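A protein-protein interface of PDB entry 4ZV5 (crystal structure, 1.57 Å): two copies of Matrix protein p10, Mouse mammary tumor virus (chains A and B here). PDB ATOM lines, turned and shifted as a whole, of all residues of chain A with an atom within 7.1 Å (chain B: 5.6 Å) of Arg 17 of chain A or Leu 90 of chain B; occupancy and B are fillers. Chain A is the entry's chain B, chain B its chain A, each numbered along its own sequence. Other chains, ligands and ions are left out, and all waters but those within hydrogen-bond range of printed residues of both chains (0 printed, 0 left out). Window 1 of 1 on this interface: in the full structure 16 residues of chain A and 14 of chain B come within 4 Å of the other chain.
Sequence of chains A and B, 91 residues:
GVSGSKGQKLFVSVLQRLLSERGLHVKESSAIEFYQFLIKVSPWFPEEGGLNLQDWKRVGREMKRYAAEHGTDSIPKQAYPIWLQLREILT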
ATOM      1  N   PHE A  11      -5.028 -10.775  14.813  1.00  0.00           N
ATOM      2  CA  PHE A  11      -4.577 -11.908  14.021  1.00  0.00           C
ATOM      3  C   PHE A  11      -5.644 -12.535  13.146  1.00  0.00           C
ATOM      4  O   PHE A  11      -5.405 -12.745  11.953  1.00  0.00           O
ATOM      5  CB  PHE A  11      -4.030 -13.014  14.933  1.00  0.00           C
ATOM      6  CG  PHE A  11      -3.652 -14.245  14.162  1.00  0.00           C
ATOM      7  CD1 PHE A  11      -2.438 -14.280  13.493  1.00  0.00           C
ATOM      8  CD2 PHE A  11      -4.558 -15.294  14.012  1.00  0.00           C
ATOM      9  CE1 PHE A  11      -2.085 -15.386  12.738  1.00  0.00           C
ATOM     10  CE2 PHE A  11      -4.216 -16.401  13.253  1.00  0.00           C
ATOM     11  CZ  PHE A  11      -2.974 -16.444  12.626  1.00  0.00           C
ATOM     12  N   VAL A  12      -6.791 -12.848  13.732  1.00  0.00           N
ATOM     13  CA  VAL A  12      -7.906 -13.437  13.016  1.00  0.00           C
ATOM     14  C   VAL A  12      -8.231 -12.515  11.840  1.00  0.00           C
ATOM     15  O   VAL A  12      -8.367 -12.991  10.707  1.00  0.00           O
ATOM     16  CB  VAL A  12      -9.111 -13.659  13.945  1.00  0.00           C
ATOM     17  CG1 VAL A  12     -10.401 -13.931  13.170  1.00  0.00           C
ATOM     18  CG2 VAL A  12      -8.772 -14.704  15.023  1.00  0.00           C
ATOM     19  N   SER A  13      -8.244 -11.203  12.072  1.00  0.00           N
ATOM     20  CA  SER A  13      -8.680 -10.279  11.004  1.00  0.00           C
ATOM     21  C   SER A  13      -7.677 -10.263   9.867  1.00  0.00           C
ATOM     22  O   SER A  13      -8.058 -10.178   8.699  1.00  0.00           O
ATOM     23  CB  SER A  13      -8.933  -8.855  11.560  1.00  0.00           C
ATOM     24  OG  SER A  13      -7.711  -8.195  11.854  1.00  0.00           O
ATOM     25  N   VAL A  14      -6.381 -10.271  10.162  1.00  0.00           N
ATOM     26  CA  VAL A  14      -5.409 -10.254   9.086  1.00  0.00           C
ATOM     27  C   VAL A  14      -5.370 -11.621   8.368  1.00  0.00           C
ATOM     28  O   VAL A  14      -5.272 -11.681   7.155  1.00  0.00           O
ATOM     29  CB  VAL A  14      -4.006  -9.923   9.612  1.00  0.00           C
ATOM     30  CG1 VAL A  14      -2.990 -10.006   8.481  1.00  0.00           C
ATOM     31  CG2 VAL A  14      -4.032  -8.513  10.222  1.00  0.00           C
ATOM     32  N   LEU A  15      -5.404 -12.711   9.133  1.00  0.00           N
ATOM     33  CA  LEU A  15      -5.416 -14.034   8.514  1.00  0.00           C
ATOM     34  C   LEU A  15      -6.624 -14.160   7.587  1.00  0.00           C
ATOM     35  O   LEU A  15      -6.523 -14.680   6.455  1.00  0.00           O
ATOM     36  CB  LEU A  15      -5.499 -15.111   9.616  1.00  0.00           C
ATOM     37  CG  LEU A  15      -5.546 -16.537   9.060  1.00  0.00           C
ATOM     38  CD1 LEU A  15      -4.172 -16.849   8.493  1.00  0.00           C
ATOM     39  CD2 LEU A  15      -5.862 -17.518  10.176  1.00  0.00           C
ATOM     40  N   GLN A  16      -7.775 -13.704   8.043  1.00  0.00           N
ATOM     41  CA  GLN A  16      -8.964 -13.934   7.228  1.00  0.00           C
ATOM     42  C   GLN A  16      -8.922 -13.077   5.936  1.00  0.00           C
ATOM     43  O   GLN A  16      -9.415 -13.516   4.882  1.00  0.00           O
ATOM     44  CB  GLN A  16     -10.242 -13.793   8.070  1.00  0.00           C
ATOM     45  CG  GLN A  16     -10.276 -14.709   9.306  1.00  0.00           C
ATOM     46  CD  GLN A  16     -11.639 -14.742  10.003  1.00  0.00           C
ATOM     47  OE1 GLN A  16     -12.368 -13.735  10.040  1.00  0.00           O
ATOM     48  NE2 GLN A  16     -11.991 -15.911  10.566  1.00  0.00           N
ATOM     49  N   ARG A  17      -8.301 -11.898   5.985  1.00  0.00           N
ATOM     50  CA  ARG A  17      -8.087 -11.079   4.796  1.00  0.00           C
ATOM     51  C   ARG A  17      -7.182 -11.812   3.814  1.00  0.00           C
ATOM     52  O   ARG A  17      -7.541 -11.978   2.631  1.00  0.00           O
ATOM     53  CB  ARG A  17      -7.467  -9.718   5.137  1.00  0.00           C
ATOM     54  CG  ARG A  17      -7.218  -8.841   3.917  1.00  0.00           C
ATOM     55  CD  ARG A  17      -6.873  -7.414   4.330  1.00  0.00           C
ATOM     56  NE  ARG A  17      -8.121  -6.783   4.743  1.00  0.00           N
ATOM     57  CZ  ARG A  17      -8.885  -6.065   3.933  1.00  0.00           C
ATOM     58  NH1 ARG A  17      -8.491  -5.821   2.684  1.00  0.00           N
ATOM     59  NH2 ARG A  17     -10.031  -5.581   4.383  1.00  0.00           N
ATOM     60  N   LEU A  18      -6.033 -12.284   4.307  1.00  0.00           N
ATOM     61  CA  LEU A  18      -5.091 -12.929   3.406  1.00  0.00           C
ATOM     62  C   LEU A  18      -5.637 -14.199   2.793  1.00  0.00           C
ATOM     63  O   LEU A  18      -5.381 -14.468   1.620  1.00  0.00           O
ATOM     64  CB  LEU A  18      -3.787 -13.233   4.151  1.00  0.00           C
ATOM     65  CG  LEU A  18      -3.011 -12.025   4.667  1.00  0.00           C
ATOM     66  CD1 LEU A  18      -1.893 -12.573   5.556  1.00  0.00           C
ATOM     67  CD2 LEU A  18      -2.447 -11.158   3.546  1.00  0.00           C
ATOM     68  N   LEU A  19      -6.350 -15.008   3.576  1.00  0.00           N
ATOM     69  CA  LEU A  19      -6.873 -16.289   3.073  1.00  0.00           C
ATOM     70  C   LEU A  19      -8.045 -16.074   2.138  1.00  0.00           C
ATOM     71  O   LEU A  19      -8.185 -16.776   1.138  1.00  0.00           O
ATOM     72  CB  LEU A  19      -7.263 -17.198   4.221  1.00  0.00           C
ATOM     73  CG  LEU A  19      -6.131 -17.818   5.064  1.00  0.00           C
ATOM     74  CD1 LEU A  19      -6.689 -18.791   6.087  1.00  0.00           C
ATOM     75  CD2 LEU A  19      -5.098 -18.535   4.199  1.00  0.00           C
ATOM     76  N   SER A  20      -8.939 -15.153   2.505  1.00  0.00           N
ATOM     77  CA  SER A  20     -10.133 -14.924   1.647  1.00  0.00           C
ATOM     78  C   SER A  20      -9.769 -14.430   0.257  1.00  0.00           C
ATOM     79  O   SER A  20     -10.459 -14.770  -0.721  1.00  0.00           O
ATOM     80  CB  SER A  20     -11.149 -13.960   2.307  1.00  0.00           C
ATOM     81  OG  SER A  20     -10.601 -12.665   2.397  1.00  0.00           O
ATOM     82  N   GLU A  21      -8.681 -13.699   0.090  1.00  0.00           N
ATOM     83  CA  GLU A  21      -8.386 -13.245  -1.264  1.00  0.00           C
ATOM     84  C   GLU A  21      -7.764 -14.362  -2.114  1.00  0.00           C
ATOM     85  O   GLU A  21      -7.561 -14.179  -3.326  1.00  0.00           O
ATOM     86  CB  GLU A  21      -7.566 -11.971  -1.304  1.00  0.00           C
ATOM     87  CG  GLU A  21      -6.239 -12.061  -0.617  1.00  0.00           C
ATOM     88  CD  GLU A  21      -5.696 -10.692  -0.220  1.00  0.00           C
ATOM     89  OE1 GLU A  21      -6.368  -9.668  -0.500  1.00  0.00           O
ATOM     90  OE2 GLU A  21      -4.606 -10.642   0.390  1.00  0.00           O
ATOM     91  N   ARG A  22      -7.483 -15.500  -1.476  1.00  0.00           N
ATOM     92  CA  ARG A  22      -7.126 -16.741  -2.204  1.00  0.00           C
ATOM     93  C   ARG A  22      -8.287 -17.735  -2.271  1.00  0.00           C
ATOM     94  O   ARG A  22      -8.088 -18.910  -2.606  1.00  0.00           O
ATOM     95  CB  ARG A  22      -5.933 -17.457  -1.551  1.00  0.00           C
ATOM     96  CG  ARG A  22      -4.582 -16.891  -1.935  1.00  0.00           C
ATOM     97  CD  ARG A  22      -4.073 -15.901  -0.935  1.00  0.00           C
ATOM     98  NE  ARG A  22      -3.106 -15.012  -1.583  1.00  0.00           N
ATOM     99  CZ  ARG A  22      -2.900 -13.745  -1.237  1.00  0.00           C
ATOM    100  NH1 ARG A  22      -3.566 -13.202  -0.204  1.00  0.00           N
ATOM    101  NH2 ARG A  22      -1.998 -13.042  -1.915  1.00  0.00           N
ATOM    102  N   LEU A  24     -10.065 -19.010   0.317  1.00  0.00           N
ATOM    103  CA  LEU A  24     -10.152 -19.928   1.444  1.00  0.00           C
ATOM    104  C   LEU A  24     -10.660 -19.228   2.694  1.00  0.00           C
ATOM    105  O   LEU A  24     -10.286 -18.107   2.991  1.00  0.00           O
ATOM    106  CB  LEU A  24      -8.805 -20.569   1.759  1.00  0.00           C
ATOM    107  CG  LEU A  24      -8.181 -21.357   0.622  1.00  0.00           C
ATOM    108  CD1 LEU A  24      -6.735 -21.653   1.014  1.00  0.00           C
ATOM    109  CD2 LEU A  24      -8.937 -22.646   0.361  1.00  0.00           C
ATOM    110  N   LEU B  18       0.221  -4.256   2.325  1.00  0.00           N
ATOM    111  CA  LEU B  18      -1.104  -3.708   1.977  1.00  0.00           C
ATOM    112  C   LEU B  18      -1.048  -2.491   1.078  1.00  0.00           C
ATOM    113  O   LEU B  18      -1.804  -2.399   0.105  1.00  0.00           O
ATOM    114  CB  LEU B  18      -1.947  -3.444   3.239  1.00  0.00           C
ATOM    115  CG  LEU B  18      -2.226  -4.689   4.080  1.00  0.00           C
ATOM    116  CD1 LEU B  18      -2.886  -4.277   5.395  1.00  0.00           C
ATOM    117  CD2 LEU B  18      -3.054  -5.716   3.306  1.00  0.00           C
ATOM    118  N   LEU B  51      -8.353  -5.426  12.224  1.00  0.00           N
ATOM    119  CA  LEU B  51      -8.116  -4.691  10.995  1.00  0.00           C
ATOM    120  C   LEU B  51      -9.445  -4.622  10.276  1.00  0.00           C
ATOM    121  O   LEU B  51      -9.751  -5.439   9.396  1.00  0.00           O
ATOM    122  CB  LEU B  51      -7.015  -5.369  10.146  1.00  0.00           C
ATOM    123  CG  LEU B  51      -6.524  -4.514   8.966  1.00  0.00           C
ATOM    124  CD1 LEU B  51      -5.981  -3.174   9.411  1.00  0.00           C
ATOM    125  CD2 LEU B  51      -5.514  -5.329   8.171  1.00  0.00           C
ATOM    126  N   ASN B  52     -10.294  -3.707  10.742  1.00  0.00           N
ATOM    127  CA  ASN B  52     -11.621  -3.531  10.207  1.00  0.00           C
ATOM    128  C   ASN B  52     -11.905  -2.033  10.243  1.00  0.00           C
ATOM    129  O   ASN B  52     -11.190  -1.286  10.909  1.00  0.00           O
ATOM    130  CB  ASN B  52     -12.652  -4.376  10.995  1.00  0.00           C
ATOM    131  CG  ASN B  52     -12.876  -3.881  12.419  1.00  0.00           C
ATOM    132  OD1 ASN B  52     -13.274  -2.734  12.641  1.00  0.00           O
ATOM    133  ND2 ASN B  52     -12.687  -4.762  13.392  1.00  0.00           N
ATOM    134  N   LEU B  53     -12.903  -1.605   9.486  1.00  0.00           N
ATOM    135  CA  LEU B  53     -13.127  -0.161   9.286  1.00  0.00           C
ATOM    136  C   LEU B  53     -13.519   0.546  10.579  1.00  0.00           C
ATOM    137  O   LEU B  53     -13.043   1.664  10.827  1.00  0.00           O
ATOM    138  CB  LEU B  53     -14.190   0.040   8.194  1.00  0.00           C
ATOM    139  CG  LEU B  53     -14.599   1.479   7.829  1.00  0.00           C
ATOM    140  CD1 LEU B  53     -13.404   2.256   7.305  1.00  0.00           C
ATOM    141  CD2 LEU B  53     -15.668   1.411   6.737  1.00  0.00           C
ATOM    142  N   TRP B  56     -10.421   0.975  12.820  1.00  0.00           N
ATOM    143  CA  TRP B  56      -9.493   1.890  12.142  1.00  0.00           C
ATOM    144  C   TRP B  56     -10.007   3.319  12.228  1.00  0.00           C
ATOM    145  O   TRP B  56      -9.211   4.256  12.383  1.00  0.00           O
ATOM    146  CB  TRP B  56      -9.233   1.424  10.695  1.00  0.00           C
ATOM    147  CG  TRP B  56      -8.005   2.046  10.123  1.00  0.00           C
ATOM    148  CD1 TRP B  56      -7.887   2.961   9.087  1.00  0.00           C
ATOM    149  CD2 TRP B  56      -6.669   1.793  10.577  1.00  0.00           C
ATOM    150  NE1 TRP B  56      -6.564   3.268   8.856  1.00  0.00           N
ATOM    151  CE2 TRP B  56      -5.782   2.625   9.748  1.00  0.00           C
ATOM    152  CE3 TRP B  56      -6.119   0.993  11.580  1.00  0.00           C
ATOM    153  CZ2 TRP B  56      -4.433   2.633   9.924  1.00  0.00           C
ATOM    154  CZ3 TRP B  56      -4.749   1.007  11.743  1.00  0.00           C
ATOM    155  CH2 TRP B  56      -3.909   1.799  10.910  1.00  0.00           C
ATOM    156  N   GLN B  85      -4.977   5.920   3.520  1.00  0.00           N
ATOM    157  CA  GLN B  85      -4.859   4.816   2.529  1.00  0.00           C
ATOM    158  C   GLN B  85      -5.323   3.482   3.108  1.00  0.00           C
ATOM    159  O   GLN B  85      -6.021   2.711   2.464  1.00  0.00           O
ATOM    160  CB  GLN B  85      -3.469   4.742   1.934  1.00  0.00           C
ATOM    161  CG  GLN B  85      -3.081   6.039   1.210  1.00  0.00           C
ATOM    162  CD  GLN B  85      -3.991   6.356   0.017  1.00  0.00           C
ATOM    163  OE1 GLN B  85      -4.596   5.470  -0.522  1.00  0.00           O
ATOM    164  NE2 GLN B  85      -4.058   7.643  -0.401  1.00  0.00           N
ATOM    165  N   LEU B  86      -4.958   3.173   4.356  1.00  0.00           N
ATOM    166  CA  LEU B  86      -5.492   1.951   4.971  1.00  0.00           C
ATOM    167  C   LEU B  86      -7.006   2.024   5.185  1.00  0.00           C
ATOM    168  O   LEU B  86      -7.695   1.042   5.071  1.00  0.00           O
ATOM    169  CB  LEU B  86      -4.776   1.647   6.291  1.00  0.00           C
ATOM    170  CG  LEU B  86      -3.301   1.355   6.101  1.00  0.00           C
ATOM    171  CD1 LEU B  86      -2.562   1.524   7.426  1.00  0.00           C
ATOM    172  CD2 LEU B  86      -3.079  -0.047   5.515  1.00  0.00           C
ATOM    173  N   ARG B  87      -7.537   3.196   5.515  1.00  0.00           N
ATOM    174  CA  ARG B  87      -8.984   3.289   5.635  1.00  0.00           C
ATOM    175  C   ARG B  87      -9.666   2.884   4.328  1.00  0.00           C
ATOM    176  O   ARG B  87     -10.654   2.132   4.356  1.00  0.00           O
ATOM    177  CB  ARG B  87      -9.469   4.679   6.068  1.00  0.00           C
ATOM    178  CG  ARG B  87     -10.974   4.684   6.360  1.00  0.00           C
ATOM    179  CD  ARG B  87     -11.558   6.056   6.654  1.00  0.00           C
ATOM    180  NE  ARG B  87     -11.401   6.984   5.537  1.00  0.00           N
ATOM    181  CZ  ARG B  87     -12.061   6.922   4.384  1.00  0.00           C
ATOM    182  NH1 ARG B  87     -12.941   5.947   4.144  1.00  0.00           N
ATOM    183  NH2 ARG B  87     -11.825   7.841   3.461  1.00  0.00           N
ATOM    184  N   GLU B  88      -9.123   3.367   3.206  1.00  0.00           N
ATOM    185  CA  GLU B  88      -9.692   3.068   1.895  1.00  0.00           C
ATOM    186  C   GLU B  88      -9.637   1.582   1.576  1.00  0.00           C
ATOM    187  O   GLU B  88     -10.611   1.013   1.062  1.00  0.00           O
ATOM    188  CB  GLU B  88      -9.009   3.893   0.820  1.00  0.00           C
ATOM    189  CG  GLU B  88      -9.571   5.288   0.802  1.00  0.00           C
ATOM    190  CD  GLU B  88     -11.055   5.256   0.458  1.00  0.00           C
ATOM    191  OE1 GLU B  88     -11.411   4.590  -0.534  1.00  0.00           O
ATOM    192  OE2 GLU B  88     -11.847   5.871   1.178  1.00  0.00           O
ATOM    193  N   ILE B  89      -8.530   0.935   1.935  1.00  0.00           N
ATOM    194  CA  ILE B  89      -8.379  -0.522   1.749  1.00  0.00           C
ATOM    195  C   ILE B  89      -9.466  -1.278   2.532  1.00  0.00           C
ATOM    196  O   ILE B  89     -10.004  -2.306   2.083  1.00  0.00           O
ATOM    197  CB  ILE B  89      -6.939  -0.945   2.153  1.00  0.00           C
ATOM    198  CG1 ILE B  89      -5.930  -0.370   1.156  1.00  0.00           C
ATOM    199  CG2 ILE B  89      -6.806  -2.461   2.388  1.00  0.00           C
ATOM    200  CD1 ILE B  89      -4.505  -0.245   1.661  1.00  0.00           C
ATOM    201  N   LEU B  90      -9.853  -0.727   3.675  1.00  0.00           N
ATOM    202  CA  LEU B  90     -10.806  -1.385   4.569  1.00  0.00           C
ATOM    203  C   LEU B  90     -12.269  -1.081   4.226  1.00  0.00           C
ATOM    204  O   LEU B  90     -13.194  -1.562   4.910  1.00  0.00           O
ATOM    205  CB  LEU B  90     -10.488  -0.998   6.019  1.00  0.00           C
ATOM    206  CG  LEU B  90      -9.133  -1.447   6.555  1.00  0.00           C
ATOM    207  CD1 LEU B  90      -9.023  -1.014   8.013  1.00  0.00           C
ATOM    208  CD2 LEU B  90      -8.900  -2.951   6.436  1.00  0.00           C
ATOM    209  N   THR B  91     -12.482  -0.301   3.159  1.00  0.00           N
ATOM    210  CA  THR B  91     -13.840   0.082   2.746  1.00  0.00           C
ATOM    211  C   THR B  91     -14.492  -0.899   1.764  1.00  0.00           C
ATOM    212  O   THR B  91     -13.827  -1.410   0.866  1.00  0.00           O
ATOM    213  CB  THR B  91     -13.870   1.518   2.191  1.00  0.00           C
ATOM    214  OG1 THR B  91     -13.427   2.424   3.211  1.00  0.00           O
ATOM    215  CG2 THR B  91     -15.288   1.910   1.773  1.00  0.00           C
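Of the printed residues of chain B, Ser 13 of chain A touches Leu 51 (2.9 Å).
Of chain B, only Ile 89 (3.8 Å) and Leu 90 (3.5 Å) come within 4 Å of Arg 17 of chain A.
Leu 18 of chain A touches none of the printed residues of chain B.
Ser 20 of chain A touches none of the printed residues of chain B.
Of the printed residues of chain A, Leu 51 of chain B touches Ser 13 (2.9 Å).
Leu 90 of chain B touches just one residue of chain A: Arg 17.
The nearest printed residue of chain A that does not touch Leu 90 of chain B is Ser 13 of chain A (7.6 Å).
The nearest printed residue of chain A that does not touch Ile 89 of chain B is Glu 21 of chain A (7.8 Å).
Among the printed residues, pairs that only touch across the chains: Arg 17 of chain A with Ile 89 of chain B (3.8 Å) and Arg 17 of chain A with Leu 90 of chain B (3.5 Å).
N of Leu 51 of chain B lies within hydrogen-bond range of OG of Ser 13 of chain A.
O of Arg 17 of chain A sits at hydrogen-bond distance from OG of Ser 20 of chain A (3.1 Å).
Of the 12 printed residues of chain B, 3 touch a printed residue of chain A.
Hydrophobic or aromatic side chains of chain B within 4 Å of the printed part of chain A: Leu 51, Ile 89 and Leu 90.
Among the printed residues, 3 pairs touch across the chains.
1 position is printed for both chains.
Of the 3 pairs that touch across the chains among the printed residues, none has its exchanged pair printed and touching as well.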
